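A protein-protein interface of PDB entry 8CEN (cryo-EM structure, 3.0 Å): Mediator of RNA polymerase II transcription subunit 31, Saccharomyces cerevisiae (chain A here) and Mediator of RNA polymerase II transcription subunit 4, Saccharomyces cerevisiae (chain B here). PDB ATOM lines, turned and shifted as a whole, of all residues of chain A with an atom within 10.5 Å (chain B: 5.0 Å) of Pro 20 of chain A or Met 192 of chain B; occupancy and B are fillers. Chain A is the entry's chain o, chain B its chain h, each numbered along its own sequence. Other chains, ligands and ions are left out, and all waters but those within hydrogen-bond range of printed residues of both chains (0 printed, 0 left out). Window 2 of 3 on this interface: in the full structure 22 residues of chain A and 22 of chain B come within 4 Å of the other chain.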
ATOM      1  N   ASN A  17      34.857 -16.264  26.257  1.00  0.00           N
ATOM      2  CA  ASN A  17      33.563 -16.508  25.633  1.00  0.00           C
ATOM      3  C   ASN A  17      32.529 -16.886  26.692  1.00  0.00           C
ATOM      4  O   ASN A  17      32.455 -18.045  27.102  1.00  0.00           O
ATOM      5  CB  ASN A  17      33.676 -17.608  24.576  1.00  0.00           C
ATOM      6  CG  ASN A  17      32.368 -17.860  23.859  1.00  0.00           C
ATOM      7  OD1 ASN A  17      31.534 -16.965  23.737  1.00  0.00           O
ATOM      8  ND2 ASN A  17      32.182 -19.083  23.377  1.00  0.00           N
ATOM      9  N   PRO A  18      31.746 -15.905  27.138  1.00  0.00           N
ATOM     10  CA  PRO A  18      30.826 -16.137  28.255  1.00  0.00           C
ATOM     11  C   PRO A  18      29.678 -17.068  27.892  1.00  0.00           C
ATOM     12  O   PRO A  18      29.288 -17.215  26.731  1.00  0.00           O
ATOM     13  CB  PRO A  18      30.305 -14.733  28.584  1.00  0.00           C
ATOM     14  CG  PRO A  18      31.337 -13.807  28.033  1.00  0.00           C
ATOM     15  CD  PRO A  18      31.834 -14.476  26.791  1.00  0.00           C
ATOM     16  N   LEU A  19      29.139 -17.701  28.930  1.00  0.00           N
ATOM     17  CA  LEU A  19      27.959 -18.535  28.789  1.00  0.00           C
ATOM     18  C   LEU A  19      26.731 -17.652  28.555  1.00  0.00           C
ATOM     19  O   LEU A  19      26.721 -16.482  28.948  1.00  0.00           O
ATOM     20  CB  LEU A  19      27.776 -19.388  30.044  1.00  0.00           C
ATOM     21  CG  LEU A  19      26.934 -20.668  30.034  1.00  0.00           C
ATOM     22  CD1 LEU A  19      27.579 -21.729  29.155  1.00  0.00           C
ATOM     23  CD2 LEU A  19      26.729 -21.190  31.445  1.00  0.00           C
ATOM     24  N   PRO A  20      25.705 -18.173  27.877  1.00  0.00           N
ATOM     25  CA  PRO A  20      24.467 -17.404  27.697  1.00  0.00           C
ATOM     26  C   PRO A  20      23.792 -17.021  29.005  1.00  0.00           C
ATOM     27  O   PRO A  20      23.894 -17.716  30.016  1.00  0.00           O
ATOM     28  CB  PRO A  20      23.586 -18.350  26.877  1.00  0.00           C
ATOM     29  CG  PRO A  20      24.549 -19.136  26.080  1.00  0.00           C
ATOM     30  CD  PRO A  20      25.787 -19.294  26.920  1.00  0.00           C
ATOM     31  N   THR A  21      23.119 -15.875  28.978  1.00  0.00           N
ATOM     32  CA  THR A  21      22.359 -15.387  30.117  1.00  0.00           C
ATOM     33  C   THR A  21      20.867 -15.575  29.876  1.00  0.00           C
ATOM     34  O   THR A  21      20.399 -15.641  28.734  1.00  0.00           O
ATOM     35  CB  THR A  21      22.659 -13.909  30.390  1.00  0.00           C
ATOM     36  OG1 THR A  21      21.936 -13.095  29.460  1.00  0.00           O
ATOM     37  CG2 THR A  21      24.144 -13.631  30.242  1.00  0.00           C
ATOM     38  N   ARG A  22      20.124 -15.662  30.984  1.00  0.00           N
ATOM     39  CA  ARG A  22      18.684 -15.891  30.917  1.00  0.00           C
ATOM     40  C   ARG A  22      17.975 -14.744  30.211  1.00  0.00           C
ATOM     41  O   ARG A  22      17.052 -14.973  29.421  1.00  0.00           O
ATOM     42  CB  ARG A  22      18.128 -16.098  32.327  1.00  0.00           C
ATOM     43  CG  ARG A  22      16.695 -16.602  32.382  1.00  0.00           C
ATOM     44  CD  ARG A  22      16.289 -16.951  33.804  1.00  0.00           C
ATOM     45  NE  ARG A  22      16.003 -15.781  34.624  1.00  0.00           N
ATOM     46  CZ  ARG A  22      15.947 -15.796  35.948  1.00  0.00           C
ATOM     47  NH1 ARG A  22      16.235 -16.886  36.639  1.00  0.00           N
ATOM     48  NH2 ARG A  22      15.602 -14.690  36.598  1.00  0.00           N
ATOM     49  N   PHE A  23      18.420 -13.508  30.463  1.00  0.00           N
ATOM     50  CA  PHE A  23      17.854 -12.336  29.798  1.00  0.00           C
ATOM     51  C   PHE A  23      18.020 -12.426  28.286  1.00  0.00           C
ATOM     52  O   PHE A  23      17.063 -12.218  27.535  1.00  0.00           O
ATOM     53  CB  PHE A  23      18.517 -11.067  30.341  1.00  0.00           C
ATOM     54  CG  PHE A  23      18.055  -9.792  29.678  1.00  0.00           C
ATOM     55  CD1 PHE A  23      16.921  -9.138  30.127  1.00  0.00           C
ATOM     56  CD2 PHE A  23      18.772  -9.232  28.626  1.00  0.00           C
ATOM     57  CE1 PHE A  23      16.497  -7.966  29.530  1.00  0.00           C
ATOM     58  CE2 PHE A  23      18.348  -8.065  28.023  1.00  0.00           C
ATOM     59  CZ  PHE A  23      17.211  -7.430  28.478  1.00  0.00           C
ATOM     60  N   GLU A  24      19.226 -12.760  27.824  1.00  0.00           N
ATOM     61  CA  GLU A  24      19.498 -12.767  26.390  1.00  0.00           C
ATOM     62  C   GLU A  24      18.794 -13.925  25.691  1.00  0.00           C
ATOM     63  O   GLU A  24      18.244 -13.752  24.595  1.00  0.00           O
ATOM     64  CB  GLU A  24      21.007 -12.815  26.156  1.00  0.00           C
ATOM     65  CG  GLU A  24      21.704 -11.535  26.589  1.00  0.00           C
ATOM     66  CD  GLU A  24      23.215 -11.627  26.544  1.00  0.00           C
ATOM     67  OE1 GLU A  24      23.741 -12.514  25.850  1.00  0.00           O
ATOM     68  OE2 GLU A  24      23.881 -10.810  27.212  1.00  0.00           O
ATOM     69  N   VAL A  25      18.787 -15.108  26.317  1.00  0.00           N
ATOM     70  CA  VAL A  25      18.093 -16.256  25.732  1.00  0.00           C
ATOM     71  C   VAL A  25      16.592 -16.003  25.665  1.00  0.00           C
ATOM     72  O   VAL A  25      15.949 -16.272  24.640  1.00  0.00           O
ATOM     73  CB  VAL A  25      18.423 -17.538  26.517  1.00  0.00           C
ATOM     74  CG1 VAL A  25      17.633 -18.715  25.977  1.00  0.00           C
ATOM     75  CG2 VAL A  25      19.903 -17.835  26.425  1.00  0.00           C
ATOM     76  N   GLU A  26      16.012 -15.464  26.741  1.00  0.00           N
ATOM     77  CA  GLU A  26      14.583 -15.188  26.743  1.00  0.00           C
ATOM     78  C   GLU A  26      14.230 -14.061  25.782  1.00  0.00           C
ATOM     79  O   GLU A  26      13.158 -14.090  25.176  1.00  0.00           O
ATOM     80  CB  GLU A  26      14.120 -14.865  28.161  1.00  0.00           C
ATOM     81  CG  GLU A  26      13.885 -16.108  28.997  1.00  0.00           C
ATOM     82  CD  GLU A  26      13.485 -15.804  30.421  1.00  0.00           C
ATOM     83  OE1 GLU A  26      13.333 -14.613  30.756  1.00  0.00           O
ATOM     84  OE2 GLU A  26      13.333 -16.759  31.211  1.00  0.00           O
ATOM     85  N   LEU A  27      15.129 -13.086  25.607  1.00  0.00           N
ATOM     86  CA  LEU A  27      14.921 -12.028  24.625  1.00  0.00           C
ATOM     87  C   LEU A  27      14.903 -12.584  23.210  1.00  0.00           C
ATOM     88  O   LEU A  27      14.027 -12.238  22.409  1.00  0.00           O
ATOM     89  CB  LEU A  27      16.012 -10.965  24.775  1.00  0.00           C
ATOM     90  CG  LEU A  27      15.923  -9.664  23.974  1.00  0.00           C
ATOM     91  CD1 LEU A  27      16.316  -8.491  24.844  1.00  0.00           C
ATOM     92  CD2 LEU A  27      16.836  -9.728  22.764  1.00  0.00           C
ATOM     93  N   GLU A  28      15.858 -13.455  22.887  1.00  0.00           N
ATOM     94  CA  GLU A  28      15.885 -14.038  21.550  1.00  0.00           C
ATOM     95  C   GLU A  28      14.669 -14.922  21.304  1.00  0.00           C
ATOM     96  O   GLU A  28      14.083 -14.882  20.214  1.00  0.00           O
ATOM     97  CB  GLU A  28      17.174 -14.822  21.343  1.00  0.00           C
ATOM     98  CG  GLU A  28      18.362 -13.949  21.019  1.00  0.00           C
ATOM     99  CD  GLU A  28      19.502 -14.748  20.449  1.00  0.00           C
ATOM    100  OE1 GLU A  28      19.694 -15.891  20.904  1.00  0.00           O
ATOM    101  OE2 GLU A  28      20.201 -14.241  19.551  1.00  0.00           O
ATOM    102  N   PHE A  29      14.245 -15.693  22.312  1.00  0.00           N
ATOM    103  CA  PHE A  29      13.069 -16.536  22.121  1.00  0.00           C
ATOM    104  C   PHE A  29      11.791 -15.716  21.996  1.00  0.00           C
ATOM    105  O   PHE A  29      10.931 -16.037  21.167  1.00  0.00           O
ATOM    106  CB  PHE A  29      12.904 -17.545  23.252  1.00  0.00           C
ATOM    107  CG  PHE A  29      11.711 -18.438  23.062  1.00  0.00           C
ATOM    108  CD1 PHE A  29      11.646 -19.303  21.982  1.00  0.00           C
ATOM    109  CD2 PHE A  29      10.627 -18.363  23.918  1.00  0.00           C
ATOM    110  CE1 PHE A  29      10.544 -20.110  21.787  1.00  0.00           C
ATOM    111  CE2 PHE A  29       9.520 -19.165  23.728  1.00  0.00           C
ATOM    112  CZ  PHE A  29       9.479 -20.039  22.660  1.00  0.00           C
ATOM    113  N   GLN A  31      11.558 -12.685  20.903  1.00  0.00           N
ATOM    114  CA  GLN A  31      11.582 -11.957  19.644  1.00  0.00           C
ATOM    115  C   GLN A  31      11.398 -12.879  18.451  1.00  0.00           C
ATOM    116  O   GLN A  31      10.914 -12.437  17.405  1.00  0.00           O
ATOM    117  CB  GLN A  31      12.881 -11.167  19.520  1.00  0.00           C
ATOM    118  CG  GLN A  31      12.896  -9.939  20.402  1.00  0.00           C
ATOM    119  CD  GLN A  31      13.727  -8.825  19.831  1.00  0.00           C
ATOM    120  OE1 GLN A  31      13.203  -7.934  19.177  1.00  0.00           O
ATOM    121  NE2 GLN A  31      15.031  -8.872  20.064  1.00  0.00           N
ATOM    122  N   SER A  32      11.750 -14.160  18.595  1.00  0.00           N
ATOM    123  CA  SER A  32      11.500 -15.141  17.546  1.00  0.00           C
ATOM    124  C   SER A  32      10.017 -15.388  17.296  1.00  0.00           C
ATOM    125  O   SER A  32       9.672 -15.974  16.265  1.00  0.00           O
ATOM    126  CB  SER A  32      12.190 -16.457  17.900  1.00  0.00           C
ATOM    127  OG  SER A  32      11.639 -17.009  19.081  1.00  0.00           O
ATOM    128  N   TYR A  38       8.441 -19.594  12.488  1.00  0.00           N
ATOM    129  CA  TYR A  38       9.028 -20.249  13.650  1.00  0.00           C
ATOM    130  C   TYR A  38       7.963 -20.716  14.634  1.00  0.00           C
ATOM    131  O   TYR A  38       8.063 -21.822  15.175  1.00  0.00           O
ATOM    132  CB  TYR A  38      10.012 -19.312  14.346  1.00  0.00           C
ATOM    133  CG  TYR A  38      10.608 -19.906  15.595  1.00  0.00           C
ATOM    134  CD1 TYR A  38      11.391 -21.046  15.534  1.00  0.00           C
ATOM    135  CD2 TYR A  38      10.364 -19.345  16.839  1.00  0.00           C
ATOM    136  CE1 TYR A  38      11.933 -21.600  16.673  1.00  0.00           C
ATOM    137  CE2 TYR A  38      10.902 -19.892  17.985  1.00  0.00           C
ATOM    138  CZ  TYR A  38      11.685 -21.020  17.896  1.00  0.00           C
ATOM    139  OH  TYR A  38      12.223 -21.570  19.035  1.00  0.00           O
ATOM    140  N   ARG B 190      22.596 -18.112  13.861  1.00  0.00           N
ATOM    141  CA  ARG B 190      23.774 -17.455  14.417  1.00  0.00           C
ATOM    142  C   ARG B 190      23.490 -16.809  15.762  1.00  0.00           C
ATOM    143  O   ARG B 190      24.436 -16.434  16.464  1.00  0.00           O
ATOM    144  CB  ARG B 190      24.321 -16.391  13.465  1.00  0.00           C
ATOM    145  CG  ARG B 190      23.444 -15.159  13.340  1.00  0.00           C
ATOM    146  CD  ARG B 190      24.033 -14.148  12.376  1.00  0.00           C
ATOM    147  NE  ARG B 190      23.210 -12.949  12.289  1.00  0.00           N
ATOM    148  CZ  ARG B 190      22.235 -12.773  11.409  1.00  0.00           C
ATOM    149  NH1 ARG B 190      21.944 -13.695  10.506  1.00  0.00           N
ATOM    150  NH2 ARG B 190      21.535 -11.641  11.432  1.00  0.00           N
ATOM    151  N   GLY B 191      22.223 -16.676  16.134  1.00  0.00           N
ATOM    152  CA  GLY B 191      21.875 -16.200  17.448  1.00  0.00           C
ATOM    153  C   GLY B 191      22.201 -17.223  18.509  1.00  0.00           C
ATOM    154  O   GLY B 191      22.575 -18.366  18.243  1.00  0.00           O
ATOM    155  N   MET B 192      22.041 -16.795  19.749  1.00  0.00           N
ATOM    156  CA  MET B 192      22.589 -17.523  20.875  1.00  0.00           C
ATOM    157  C   MET B 192      21.533 -18.272  21.676  1.00  0.00           C
ATOM    158  O   MET B 192      21.878 -18.956  22.644  1.00  0.00           O
ATOM    159  CB  MET B 192      23.382 -16.546  21.737  1.00  0.00           C
ATOM    160  CG  MET B 192      22.559 -15.470  22.375  1.00  0.00           C
ATOM    161  SD  MET B 192      23.666 -14.441  23.321  1.00  0.00           S
ATOM    162  CE  MET B 192      24.054 -15.530  24.657  1.00  0.00           C
ATOM    163  N   LEU B 193      20.262 -18.190  21.276  1.00  0.00           N
ATOM    164  CA  LEU B 193      19.294 -19.206  21.674  1.00  0.00           C
ATOM    165  C   LEU B 193      19.662 -20.558  21.071  1.00  0.00           C
ATOM    166  O   LEU B 193      19.467 -21.609  21.699  1.00  0.00           O
ATOM    167  CB  LEU B 193      17.889 -18.779  21.247  1.00  0.00           C
ATOM    168  CG  LEU B 193      16.738 -19.788  21.320  1.00  0.00           C
ATOM    169  CD1 LEU B 193      16.541 -20.288  22.738  1.00  0.00           C
ATOM    170  CD2 LEU B 193      15.453 -19.180  20.780  1.00  0.00           C
ATOM    171  N   ALA B 194      20.219 -20.542  19.855  1.00  0.00           N
ATOM    172  CA  ALA B 194      20.659 -21.772  19.208  1.00  0.00           C
ATOM    173  C   ALA B 194      21.776 -22.452  19.993  1.00  0.00           C
ATOM    174  O   ALA B 194      21.758 -23.675  20.170  1.00  0.00           O
ATOM    175  CB  ALA B 194      21.111 -21.478  17.779  1.00  0.00           C
ATOM    176  N   MET B 195      22.754 -21.683  20.477  1.00  0.00           N
ATOM    177  CA  MET B 195      23.790 -22.288  21.304  1.00  0.00           C
ATOM    178  C   MET B 195      23.341 -22.468  22.745  1.00  0.00           C
ATOM    179  O   MET B 195      23.957 -23.247  23.477  1.00  0.00           O
ATOM    180  CB  MET B 195      25.078 -21.463  21.271  1.00  0.00           C
ATOM    181  CG  MET B 195      24.963 -20.087  21.878  1.00  0.00           C
ATOM    182  SD  MET B 195      26.523 -19.194  21.816  1.00  0.00           S
ATOM    183  CE  MET B 195      27.464 -20.078  23.056  1.00  0.00           C
ATOM    184  N   ALA B 196      22.277 -21.777  23.164  1.00  0.00           N
ATOM    185  CA  ALA B 196      21.644 -22.095  24.439  1.00  0.00           C
ATOM    186  C   ALA B 196      21.041 -23.491  24.405  1.00  0.00           C
ATOM    187  O   ALA B 196      21.028 -24.199  25.419  1.00  0.00           O
ATOM    188  CB  ALA B 196      20.572 -21.058  24.763  1.00  0.00           C
ATOM    189  N   LEU B 203      23.064 -24.099  31.483  1.00  0.00           N
ATOM    190  CA  LEU B 203      22.149 -23.013  31.819  1.00  0.00           C
ATOM    191  C   LEU B 203      21.127 -23.415  32.874  1.00  0.00           C
ATOM    192  O   LEU B 203      20.539 -22.540  33.518  1.00  0.00           O
ATOM    193  CB  LEU B 203      21.419 -22.533  30.567  1.00  0.00           C
ATOM    194  CG  LEU B 203      22.301 -21.975  29.454  1.00  0.00           C
ATOM    195  CD1 LEU B 203      21.451 -21.512  28.292  1.00  0.00           C
ATOM    196  CD2 LEU B 203      23.162 -20.854  29.975  1.00  0.00           C
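Asn 17 of chain A touches none of the printed residues of chain B.
Of the printed residues of chain B, Leu 19 of chain A touches Leu 203.
Of chain B, only Met 192 (3.6 Å) and Leu 203 (3.2 Å) come within 4 Å of Pro 20 of chain A.
Printed residues of chain B within 4 Å of Glu 24 of chain A: Met 192 (3.2 Å).
Printed residues of chain B within 4 Å of Val 25 of chain A: Leu 193 (3.8 Å) and Ala 196 (3.7 Å).
Printed residues of chain B within 4 Å of Glu 28 of chain A: Gly 191 (3.3 Å), Met 192 (2.8 Å) and Leu 193 (2.4 Å).
Printed residues of chain B within 4 Å of Phe 29 of chain A: Leu 193.
Gln 31 of chain A touches none of the printed residues of chain B.
Of chain A, only Glu 28 comes within 4 Å of Gly 191 of chain B.
Of chain A, only Pro 20 (3.6 Å), Glu 24 (3.2 Å) and Glu 28 (2.8 Å) come within 4 Å of Met 192 of chain B.
Leu 193 of chain B touches just these residues of chain A: Val 25, Glu 28 and Phe 29.
No residue of chain A comes within 4 Å of Met 195 of chain B.
Of chain A, only Val 25 (3.7 Å) comes within 4 Å of Ala 196 of chain B.
The nearest residue of chain B that does not touch Pro 20 of chain A is Met 195 of chain B (4.3 Å).
The nearest printed residue of chain A that does not touch Met 192 of chain B is Val 25 of chain A (4.4 Å).
Leu 203 of chain B touches Leu 19 of chain A (CD2 to CG, 3.8 Å).
Met 192 of chain B touches Pro 20 of chain A.
Leu 203 of chain B touches Pro 20 of chain A (CD2 to O, 3.2 Å).
CD1 of Leu 193 of chain B touches CG1 of Val 25 of chain A, at 3.8 Å.
Ala 196 of chain B touches Val 25 of chain A (CB to CG2, 3.7 Å).
Glu 28 of chain A touches Gly 191 of chain B (OE2 to CA, 3.3 Å).
CA of Phe 29 of chain A touches CD2 of Leu 193 of chain B, 3.8 Å away.
OE1 of Glu 28 of chain A is in hydrogen-bond range of N of Met 192 of chain B (2.8 Å).
OE1 of Glu 24 of chain A sits close to SD of Met 192 of chain B (3.2 Å).
The side-chain carboxylate of Glu 28 of chain A sits close to the backbone NH of Leu 193 of chain B (2.4 Å).
The side-chain hydroxyl (OG) of Ser 32 of chain A sits close to the backbone carbonyl oxygen (O) of Glu 28 of chain A, 3.4 Å away.
O of Phe 29 of chain A lies within hydrogen-bond range of OG of Ser 32 of chain A (2.4 Å).
The side-chain hydroxyl of Thr 21 of chain A is in hydrogen-bond range of the backbone NH of Glu 24 of chain A, 3.2 Å away.
Hydrophobic or aromatic side chains of chain B within 4 Å of the printed part of chain A: Met 192, Leu 193, Ala 196 and Leu 203.
Among the printed residues, no Asp or Glu carboxylate lies within 4 Å of a Lys or Arg side-chain nitrogen of the other chain.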
